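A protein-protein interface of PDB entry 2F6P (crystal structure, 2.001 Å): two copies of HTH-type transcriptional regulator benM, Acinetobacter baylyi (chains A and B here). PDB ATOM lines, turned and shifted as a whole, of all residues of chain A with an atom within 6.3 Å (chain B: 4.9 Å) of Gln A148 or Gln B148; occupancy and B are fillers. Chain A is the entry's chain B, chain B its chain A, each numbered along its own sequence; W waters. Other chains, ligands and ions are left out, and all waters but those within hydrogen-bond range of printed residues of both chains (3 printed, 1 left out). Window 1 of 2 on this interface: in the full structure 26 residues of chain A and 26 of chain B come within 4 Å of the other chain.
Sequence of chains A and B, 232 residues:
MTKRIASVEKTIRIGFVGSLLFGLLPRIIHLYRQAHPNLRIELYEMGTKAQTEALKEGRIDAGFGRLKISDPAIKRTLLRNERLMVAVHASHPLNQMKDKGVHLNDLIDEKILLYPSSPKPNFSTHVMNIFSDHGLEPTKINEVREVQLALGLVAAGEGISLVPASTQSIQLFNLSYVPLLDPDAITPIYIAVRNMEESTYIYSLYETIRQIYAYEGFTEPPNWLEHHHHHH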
ATOM      1  N   VAL A  17     -16.027   3.498  21.029  1.00  0.00           N
ATOM      2  CA  VAL A  17     -17.181   4.265  21.494  1.00  0.00           C
ATOM      3  C   VAL A  17     -18.394   3.371  21.267  1.00  0.00           C
ATOM      4  O   VAL A  17     -18.539   2.788  20.191  1.00  0.00           O
ATOM      5  CB  VAL A  17     -17.343   5.587  20.709  1.00  0.00           C
ATOM      6  CG1 VAL A  17     -18.631   6.298  21.110  1.00  0.00           C
ATOM      7  CG2 VAL A  17     -16.146   6.486  20.943  1.00  0.00           C
ATOM      8  N   GLY A  18     -19.242   3.247  22.282  1.00  0.00           N
ATOM      9  CA  GLY A  18     -20.368   2.304  22.258  1.00  0.00           C
ATOM     10  C   GLY A  18     -21.312   2.413  21.072  1.00  0.00           C
ATOM     11  O   GLY A  18     -21.756   1.398  20.526  1.00  0.00           O
ATOM     12  N   SER A  19     -21.617   3.643  20.668  1.00  0.00           N
ATOM     13  CA  SER A  19     -22.563   3.889  19.578  1.00  0.00           C
ATOM     14  C   SER A  19     -22.065   3.439  18.199  1.00  0.00           C
ATOM     15  O   SER A  19     -22.866   3.305  17.270  1.00  0.00           O
ATOM     16  CB  SER A  19     -22.917   5.375  19.517  1.00  0.00           C
ATOM     17  OG  SER A  19     -21.780   6.134  19.143  1.00  0.00           O
ATOM     18  N   LEU A  20     -20.758   3.218  18.057  1.00  0.00           N
ATOM     19  CA  LEU A  20     -20.211   2.653  16.820  1.00  0.00           C
ATOM     20  C   LEU A  20     -20.702   1.222  16.556  1.00  0.00           C
ATOM     21  O   LEU A  20     -20.570   0.712  15.440  1.00  0.00           O
ATOM     22  CB  LEU A  20     -18.684   2.687  16.842  1.00  0.00           C
ATOM     23  CG  LEU A  20     -18.004   4.059  16.830  1.00  0.00           C
ATOM     24  CD1 LEU A  20     -16.493   3.885  16.946  1.00  0.00           C
ATOM     25  CD2 LEU A  20     -18.359   4.842  15.568  1.00  0.00           C
ATOM     26  N   LEU A  21     -21.268   0.572  17.572  1.00  0.00           N
ATOM     27  CA  LEU A  21     -21.868  -0.753  17.393  1.00  0.00           C
ATOM     28  C   LEU A  21     -23.122  -0.721  16.506  1.00  0.00           C
ATOM     29  O   LEU A  21     -23.555  -1.762  16.007  1.00  0.00           O
ATOM     30  CB  LEU A  21     -22.202  -1.381  18.750  1.00  0.00           C
ATOM     31  CG  LEU A  21     -21.003  -1.733  19.631  1.00  0.00           C
ATOM     32  CD1 LEU A  21     -21.505  -2.171  21.000  1.00  0.00           C
ATOM     33  CD2 LEU A  21     -20.141  -2.810  18.995  1.00  0.00           C
ATOM     34  N   PHE A  22     -23.684   0.471  16.294  1.00  0.00           N
ATOM     35  CA  PHE A  22     -24.793   0.653  15.358  1.00  0.00           C
ATOM     36  C   PHE A  22     -24.338   0.735  13.892  1.00  0.00           C
ATOM     37  O   PHE A  22     -25.174   0.717  12.989  1.00  0.00           O
ATOM     38  CB  PHE A  22     -25.592   1.905  15.720  1.00  0.00           C
ATOM     39  CG  PHE A  22     -26.221   1.851  17.089  1.00  0.00           C
ATOM     40  CD1 PHE A  22     -27.101   0.828  17.423  1.00  0.00           C
ATOM     41  CD2 PHE A  22     -25.948   2.829  18.038  1.00  0.00           C
ATOM     42  CE1 PHE A  22     -27.686   0.774  18.677  1.00  0.00           C
ATOM     43  CE2 PHE A  22     -26.525   2.780  19.295  1.00  0.00           C
ATOM     44  CZ  PHE A  22     -27.399   1.753  19.616  1.00  0.00           C
ATOM     45  N   GLU A  45     -15.717  -0.958  25.793  1.00  0.00           N
ATOM     46  CA  GLU A  45     -16.413   0.273  25.497  1.00  0.00           C
ATOM     47  C   GLU A  45     -15.748   1.410  26.279  1.00  0.00           C
ATOM     48  O   GLU A  45     -15.582   1.325  27.506  1.00  0.00           O
ATOM     49  CB  GLU A  45     -17.880   0.143  25.895  1.00  0.00           C
ATOM     50  CG  GLU A  45     -18.733   1.331  25.522  1.00  0.00           C
ATOM     51  CD  GLU A  45     -20.124   1.267  26.134  1.00  0.00           C
ATOM     52  OE1 GLU A  45     -20.289   0.650  27.210  1.00  0.00           O
ATOM     53  OE2 GLU A  45     -21.055   1.837  25.536  1.00  0.00           O
ATOM     54  N   ARG A 145     -27.341  11.631  28.336  1.00  0.00           N
ATOM     55  CA  ARG A 145     -26.289  10.637  28.575  1.00  0.00           C
ATOM     56  C   ARG A 145     -25.715   9.974  27.325  1.00  0.00           C
ATOM     57  O   ARG A 145     -24.500   9.791  27.222  1.00  0.00           O
ATOM     58  CB  ARG A 145     -26.808   9.551  29.524  1.00  0.00           C
ATOM     59  CG  ARG A 145     -25.785   8.479  29.874  1.00  0.00           C
ATOM     60  CD  ARG A 145     -26.155   7.738  31.150  1.00  0.00           C
ATOM     61  NE  ARG A 145     -27.242   6.774  30.963  1.00  0.00           N
ATOM     62  CZ  ARG A 145     -27.095   5.530  30.501  1.00  0.00           C
ATOM     63  NH1 ARG A 145     -25.904   5.062  30.146  1.00  0.00           N
ATOM     64  NH2 ARG A 145     -28.157   4.743  30.384  1.00  0.00           N
ATOM     65  N   GLU A 146     -26.586   9.587  26.399  1.00  0.00           N
ATOM     66  CA  GLU A 146     -26.170   8.839  25.215  1.00  0.00           C
ATOM     67  C   GLU A 146     -27.238   8.928  24.126  1.00  0.00           C
ATOM     68  O   GLU A 146     -28.352   9.382  24.379  1.00  0.00           O
ATOM     69  CB  GLU A 146     -25.868   7.370  25.579  1.00  0.00           C
ATOM     70  CG  GLU A 146     -27.052   6.596  26.179  1.00  0.00           C
ATOM     71  CD  GLU A 146     -26.696   5.177  26.613  1.00  0.00           C
ATOM     72  OE1 GLU A 146     -25.497   4.821  26.614  1.00  0.00           O
ATOM     73  OE2 GLU A 146     -27.624   4.414  26.960  1.00  0.00           O
ATOM     74  N   VAL A 147     -26.897   8.488  22.918  1.00  0.00           N
ATOM     75  CA  VAL A 147     -27.765   8.710  21.760  1.00  0.00           C
ATOM     76  C   VAL A 147     -29.129   8.017  21.874  1.00  0.00           C
ATOM     77  O   VAL A 147     -30.139   8.588  21.457  1.00  0.00           O
ATOM     78  CB  VAL A 147     -27.062   8.339  20.419  1.00  0.00           C
ATOM     79  CG1 VAL A 147     -26.767   6.849  20.322  1.00  0.00           C
ATOM     80  CG2 VAL A 147     -27.892   8.809  19.234  1.00  0.00           C
ATOM     81  N   GLN A 148     -29.174   6.811  22.435  1.00  0.00           N
ATOM     82  CA  GLN A 148     -30.445   6.080  22.513  1.00  0.00           C
ATOM     83  C   GLN A 148     -31.443   6.756  23.466  1.00  0.00           C
ATOM     84  O   GLN A 148     -32.651   6.715  23.230  1.00  0.00           O
ATOM     85  CB  GLN A 148     -30.231   4.594  22.851  1.00  0.00           C
ATOM     86  CG  GLN A 148     -29.772   4.274  24.259  1.00  0.00           C
ATOM     87  CD  GLN A 148     -29.425   2.802  24.428  1.00  0.00           C
ATOM     88  OE1 GLN A 148     -28.775   2.203  23.570  1.00  0.00           O
ATOM     89  NE2 GLN A 148     -29.860   2.210  25.535  1.00  0.00           N
ATOM     90  N   LEU A 149     -30.934   7.399  24.517  1.00  0.00           N
ATOM     91  CA  LEU A 149     -31.763   8.215  25.410  1.00  0.00           C
ATOM     92  C   LEU A 149     -32.298   9.451  24.678  1.00  0.00           C
ATOM     93  O   LEU A 149     -33.455   9.827  24.843  1.00  0.00           O
ATOM     94  CB  LEU A 149     -30.954   8.671  26.625  1.00  0.00           C
ATOM     95  CG  LEU A 149     -31.638   8.788  27.993  1.00  0.00           C
ATOM     96  CD1 LEU A 149     -30.813   9.697  28.880  1.00  0.00           C
ATOM     97  CD2 LEU A 149     -33.068   9.290  27.936  1.00  0.00           C
ATOM     98  N   ALA A 150     -31.440  10.093  23.890  1.00  0.00           N
ATOM     99  CA  ALA A 150     -31.855  11.252  23.091  1.00  0.00           C
ATOM    100  C   ALA A 150     -32.986  10.893  22.126  1.00  0.00           C
ATOM    101  O   ALA A 150     -33.943  11.653  21.975  1.00  0.00           O
ATOM    102  CB  ALA A 150     -30.672  11.827  22.331  1.00  0.00           C
ATOM    103  N   LEU A 151     -32.882   9.729  21.488  1.00  0.00           N
ATOM    104  CA  LEU A 151     -33.897   9.283  20.542  1.00  0.00           C
ATOM    105  C   LEU A 151     -35.242   9.010  21.211  1.00  0.00           C
ATOM    106  O   LEU A 151     -36.288   9.351  20.664  1.00  0.00           O
ATOM    107  CB  LEU A 151     -33.435   8.022  19.809  1.00  0.00           C
ATOM    108  CG  LEU A 151     -32.192   8.167  18.931  1.00  0.00           C
ATOM    109  CD1 LEU A 151     -31.795   6.815  18.360  1.00  0.00           C
ATOM    110  CD2 LEU A 151     -32.413   9.178  17.821  1.00  0.00           C
ATOM    111  N   GLY A 152     -35.206   8.372  22.378  1.00  0.00           N
ATOM    112  CA  GLY A 152     -36.415   8.082  23.138  1.00  0.00           C
ATOM    113  C   GLY A 152     -37.108   9.346  23.608  1.00  0.00           C
ATOM    114  O   GLY A 152     -38.339   9.423  23.600  1.00  0.00           O
ATOM    115  N   LEU A 153     -36.310  10.330  24.024  1.00  0.00           N
ATOM    116  CA  LEU A 153     -36.812  11.654  24.420  1.00  0.00           C
ATOM    117  C   LEU A 153     -37.430  12.413  23.235  1.00  0.00           C
ATOM    118  O   LEU A 153     -38.486  13.032  23.375  1.00  0.00           O
ATOM    119  CB  LEU A 153     -35.684  12.482  25.056  1.00  0.00           C
ATOM    120  CG  LEU A 153     -35.463  12.414  26.576  1.00  0.00           C
ATOM    121  CD1 LEU A 153     -35.794  11.056  27.168  1.00  0.00           C
ATOM    122  CD2 LEU A 153     -34.034  12.814  26.920  1.00  0.00           C
ATOM    123  N   ILE A 170     -31.680   2.169  14.870  1.00  0.00           N
ATOM    124  CA  ILE A 170     -32.777   2.317  15.821  1.00  0.00           C
ATOM    125  C   ILE A 170     -33.985   2.967  15.138  1.00  0.00           C
ATOM    126  O   ILE A 170     -33.877   4.066  14.604  1.00  0.00           O
ATOM    127  CB  ILE A 170     -32.353   3.192  17.026  1.00  0.00           C
ATOM    128  CG1 ILE A 170     -31.098   2.607  17.693  1.00  0.00           C
ATOM    129  CG2 ILE A 170     -33.532   3.341  18.012  1.00  0.00           C
ATOM    130  CD1 ILE A 170     -30.447   3.507  18.755  1.00  0.00           C
ATOM    131  N   LEU A 172     -38.043   3.909  16.053  1.00  0.00           N
ATOM    132  CA  LEU A 172     -39.077   4.013  17.076  1.00  0.00           C
ATOM    133  C   LEU A 172     -40.344   4.608  16.475  1.00  0.00           C
ATOM    134  O   LEU A 172     -40.284   5.379  15.516  1.00  0.00           O
ATOM    135  CB  LEU A 172     -38.599   4.907  18.225  1.00  0.00           C
ATOM    136  CG  LEU A 172     -37.273   4.544  18.898  1.00  0.00           C
ATOM    137  CD1 LEU A 172     -36.997   5.502  20.059  1.00  0.00           C
ATOM    138  CD2 LEU A 172     -37.278   3.085  19.375  1.00  0.00           C
ATOM    139  N   LEU B  21     -37.833   2.864  26.602  1.00  0.00           N
ATOM    140  CA  LEU B  21     -37.845   3.800  25.472  1.00  0.00           C
ATOM    141  C   LEU B  21     -37.996   3.118  24.099  1.00  0.00           C
ATOM    142  O   LEU B  21     -38.314   3.789  23.113  1.00  0.00           O
ATOM    143  CB  LEU B  21     -36.580   4.668  25.475  1.00  0.00           C
ATOM    144  CG  LEU B  21     -36.428   5.671  26.630  1.00  0.00           C
ATOM    145  CD1 LEU B  21     -35.152   6.499  26.464  1.00  0.00           C
ATOM    146  CD2 LEU B  21     -37.639   6.580  26.737  1.00  0.00           C
ATOM    147  N   PHE B  22     -37.768   1.806  24.033  1.00  0.00           N
ATOM    148  CA  PHE B  22     -37.918   1.050  22.778  1.00  0.00           C
ATOM    149  C   PHE B  22     -39.341   0.535  22.539  1.00  0.00           C
ATOM    150  O   PHE B  22     -39.633  -0.007  21.465  1.00  0.00           O
ATOM    151  CB  PHE B  22     -36.945  -0.136  22.748  1.00  0.00           C
ATOM    152  CG  PHE B  22     -35.498   0.262  22.835  1.00  0.00           C
ATOM    153  CD1 PHE B  22     -34.939   1.106  21.887  1.00  0.00           C
ATOM    154  CD2 PHE B  22     -34.691  -0.213  23.857  1.00  0.00           C
ATOM    155  CE1 PHE B  22     -33.600   1.485  21.966  1.00  0.00           C
ATOM    156  CE2 PHE B  22     -33.349   0.158  23.939  1.00  0.00           C
ATOM    157  CZ  PHE B  22     -32.807   1.006  22.993  1.00  0.00           C
ATOM    158  N   GLU B 146     -25.079  -2.688  29.089  1.00  0.00           N
ATOM    159  CA  GLU B 146     -26.453  -2.428  28.671  1.00  0.00           C
ATOM    160  C   GLU B 146     -26.766  -3.170  27.372  1.00  0.00           C
ATOM    161  O   GLU B 146     -25.886  -3.802  26.774  1.00  0.00           O
ATOM    162  CB  GLU B 146     -26.713  -0.914  28.538  1.00  0.00           C
ATOM    163  CG  GLU B 146     -25.742  -0.160  27.626  1.00  0.00           C
ATOM    164  CD  GLU B 146     -26.189   1.273  27.322  1.00  0.00           C
ATOM    165  OE1 GLU B 146     -26.947   1.872  28.124  1.00  0.00           O
ATOM    166  OE2 GLU B 146     -25.777   1.803  26.266  1.00  0.00           O
ATOM    167  N   VAL B 147     -28.027  -3.100  26.958  1.00  0.00           N
ATOM    168  CA  VAL B 147     -28.531  -3.894  25.838  1.00  0.00           C
ATOM    169  C   VAL B 147     -27.787  -3.665  24.513  1.00  0.00           C
ATOM    170  O   VAL B 147     -27.487  -4.632  23.818  1.00  0.00           O
ATOM    171  CB  VAL B 147     -30.068  -3.698  25.645  1.00  0.00           C
ATOM    172  CG1 VAL B 147     -30.415  -2.250  25.283  1.00  0.00           C
ATOM    173  CG2 VAL B 147     -30.607  -4.670  24.608  1.00  0.00           C
ATOM    174  N   GLN B 148     -27.473  -2.414  24.173  1.00  0.00           N
ATOM    175  CA  GLN B 148     -26.781  -2.124  22.907  1.00  0.00           C
ATOM    176  C   GLN B 148     -25.429  -2.841  22.823  1.00  0.00           C
ATOM    177  O   GLN B 148     -25.019  -3.282  21.746  1.00  0.00           O
ATOM    178  CB  GLN B 148     -26.602  -0.611  22.676  1.00  0.00           C
ATOM    179  CG  GLN B 148     -25.439   0.039  23.429  1.00  0.00           C
ATOM    180  CD  GLN B 148     -25.146   1.452  22.960  1.00  0.00           C
ATOM    181  OE1 GLN B 148     -24.038   1.752  22.516  1.00  0.00           O
ATOM    182  NE2 GLN B 148     -26.137   2.325  23.054  1.00  0.00           N
ATOM    183  N   LEU B 149     -24.746  -2.959  23.962  1.00  0.00           N
ATOM    184  CA  LEU B 149     -23.457  -3.658  24.012  1.00  0.00           C
ATOM    185  C   LEU B 149     -23.650  -5.153  23.737  1.00  0.00           C
ATOM    186  O   LEU B 149     -22.895  -5.747  22.968  1.00  0.00           O
ATOM    187  CB  LEU B 149     -22.757  -3.448  25.360  1.00  0.00           C
ATOM    188  CG  LEU B 149     -21.265  -3.111  25.281  1.00  0.00           C
ATOM    189  CD1 LEU B 149     -20.679  -3.049  26.674  1.00  0.00           C
ATOM    190  CD2 LEU B 149     -20.488  -4.106  24.417  1.00  0.00           C
ATOM    191  N   ALA B 150     -24.668  -5.748  24.358  1.00  0.00           N
ATOM    192  CA  ALA B 150     -24.988  -7.158  24.139  1.00  0.00           C
ATOM    193  C   ALA B 150     -25.313  -7.440  22.669  1.00  0.00           C
ATOM    194  O   ALA B 150     -24.811  -8.402  22.095  1.00  0.00           O
ATOM    195  CB  ALA B 150     -26.145  -7.586  25.028  1.00  0.00           C
ATOM    196  N   LEU B 151     -26.142  -6.589  22.068  1.00  0.00           N
ATOM    197  CA  LEU B 151     -26.558  -6.761  20.669  1.00  0.00           C
ATOM    198  C   LEU B 151     -25.390  -6.632  19.700  1.00  0.00           C
ATOM    199  O   LEU B 151     -25.250  -7.437  18.769  1.00  0.00           O
ATOM    200  CB  LEU B 151     -27.633  -5.736  20.299  1.00  0.00           C
ATOM    201  CG  LEU B 151     -28.936  -5.798  21.093  1.00  0.00           C
ATOM    202  CD1 LEU B 151     -29.851  -4.652  20.682  1.00  0.00           C
ATOM    203  CD2 LEU B 151     -29.620  -7.139  20.907  1.00  0.00           C
ATOM    204  N   GLY B 152     -24.564  -5.610  19.921  1.00  0.00           N
ATOM    205  CA  GLY B 152     -23.351  -5.400  19.136  1.00  0.00           C
ATOM    206  C   GLY B 152     -22.383  -6.566  19.220  1.00  0.00           C
ATOM    207  O   GLY B 152     -21.758  -6.930  18.218  1.00  0.00           O
HETATM  208  O   HOH W   1     -28.018   0.110  25.329  1.00  0.00           O
HETATM  209  O   HOH W   2     -24.297   4.553  22.716  1.00  0.00           O
HETATM  210  O   HOH W   3     -26.058   1.995  31.317  1.00  0.00           O
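Water W1 lies within hydrogen-bond range of NE2 of Gln A148, N of Gln B148 and OE2 of Glu B146.
Water W2 lies within hydrogen-bond range of the side-chain amide oxygen of Gln B148 (2.8 Å) and the backbone NH of Ser A19 (3.5 Å).
Water W3 lies within hydrogen-bond range of the guanidinium group of Arg A145 (3.3 Å) and the side-chain carboxylate of Glu B146 (3.3 Å).
Phe A22 touches Gln B148, but with the chains exchanged Gln A148 does not touch Phe B22 (4.1 Å).
Glu A146 touches its own counterpart, Glu B146.
Gln A148 touches Glu B146, but with the chains exchanged Glu A146 does not touch Gln B148 (4.4 Å).
Gly A152 touches Leu B21, but with the chains exchanged Leu A21 does not touch Gly B152 (4.1 Å).
9 positions are printed for both chains.
Of the 14 pairs that touch across the chains among the printed residues, 4 have their exchanged pair printed and touching as well.
Ser A19 touches Gln B148.
Leu A21 touches Gln B148 (CD1 to O, 3.8 Å).
CD1 of Leu A21 touches CA of Leu B149 (3.9 Å).
Phe A22 touches Gln B148.
OE1 of Glu A45 touches CD1 of Leu B149 (3.8 Å).
Gln A148 touches Glu B146.
Leu A149 touches Leu B21.
Gly A152 touches Leu B21 (CA to CD1, 3.9 Å).
Leu A172 touches Leu B21.
Leu A172 touches Phe B22.
Of the 18 printed residues of chain A, 11 touch a printed residue of chain B.
Printed residues of chain A that touch a printed residue of chain B: Gly A18, Ser A19, Leu A21, Phe A22, Glu A45, Arg A145, Glu A146, Gln A148, Leu A149, Gly A152 and Leu A172.
Hydrophobic or aromatic side chains of chain A that line the printed part of chain B: Leu A21, Phe A22, Leu A149 and Leu A172.
Of the 9 printed residues of chain B, 5 touch a printed residue of chain A.
Printed residues of chain B that touch a printed residue of chain A: Leu B21, Phe B22, Glu B146, Gln B148 and Leu B149.
Hydrophobic or aromatic side chains of chain B within 4 Å of the printed part of chain A: Leu B21, Phe B22 and Leu B149.
Among the printed residues, 14 pairs touch across the chains.
Gln A148 touches just these residues of chain B: Glu B146 (3.9 Å) and Gln B148 (2.7 Å).
Gln B148 touches just these residues of chain A: Gly A18 (3.0 Å), Ser A19 (3.6 Å), Leu A21 (3.8 Å), Phe A22 (3.7 Å) and Gln A148 (2.7 Å).
Of the printed residues of chain B, Leu A21 touches Gln B148 and Leu B149.
Of the printed residues of chain B, Glu A45 touches Leu B149 (3.8 Å).
Of the printed residues of chain B, Gly A18 touches Gln B148 (3.0 Å).
Of the printed residues of chain B, Leu A149 touches Leu B21.
The nearest printed residue of chain B that does not touch Gly A18 is Leu B149 (6.3 Å).
The side-chain amide nitrogen (NE2) of Gln A148 lies within hydrogen-bond range of the side-chain carboxylate (OE2) of Glu A146 (3.4 Å).
NH2 of Arg A145 is in salt-bridge range of OE2 of Glu A146 (3.5 Å).
The side-chain carboxylate of Glu B146 sits at hydrogen-bond distance from the side-chain amide nitrogen of Gln B148.
The side-chain amide oxygen (OE1) of Gln A148 sits at hydrogen-bond distance from the side-chain amide nitrogen (NE2) of Gln B148, 2.7 Å away.
The backbone carbonyl oxygen of Gly A18 sits close to the side-chain amide oxygen of Gln B148, 3.0 Å away.
The side-chain carboxylate of Glu B146 sits close to the side-chain carboxylate of Glu A146 (2.9 Å).
The guanidinium group of Arg A145 lies within salt-bridge range of the side-chain carboxylate of Glu B146 (3.8 Å).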
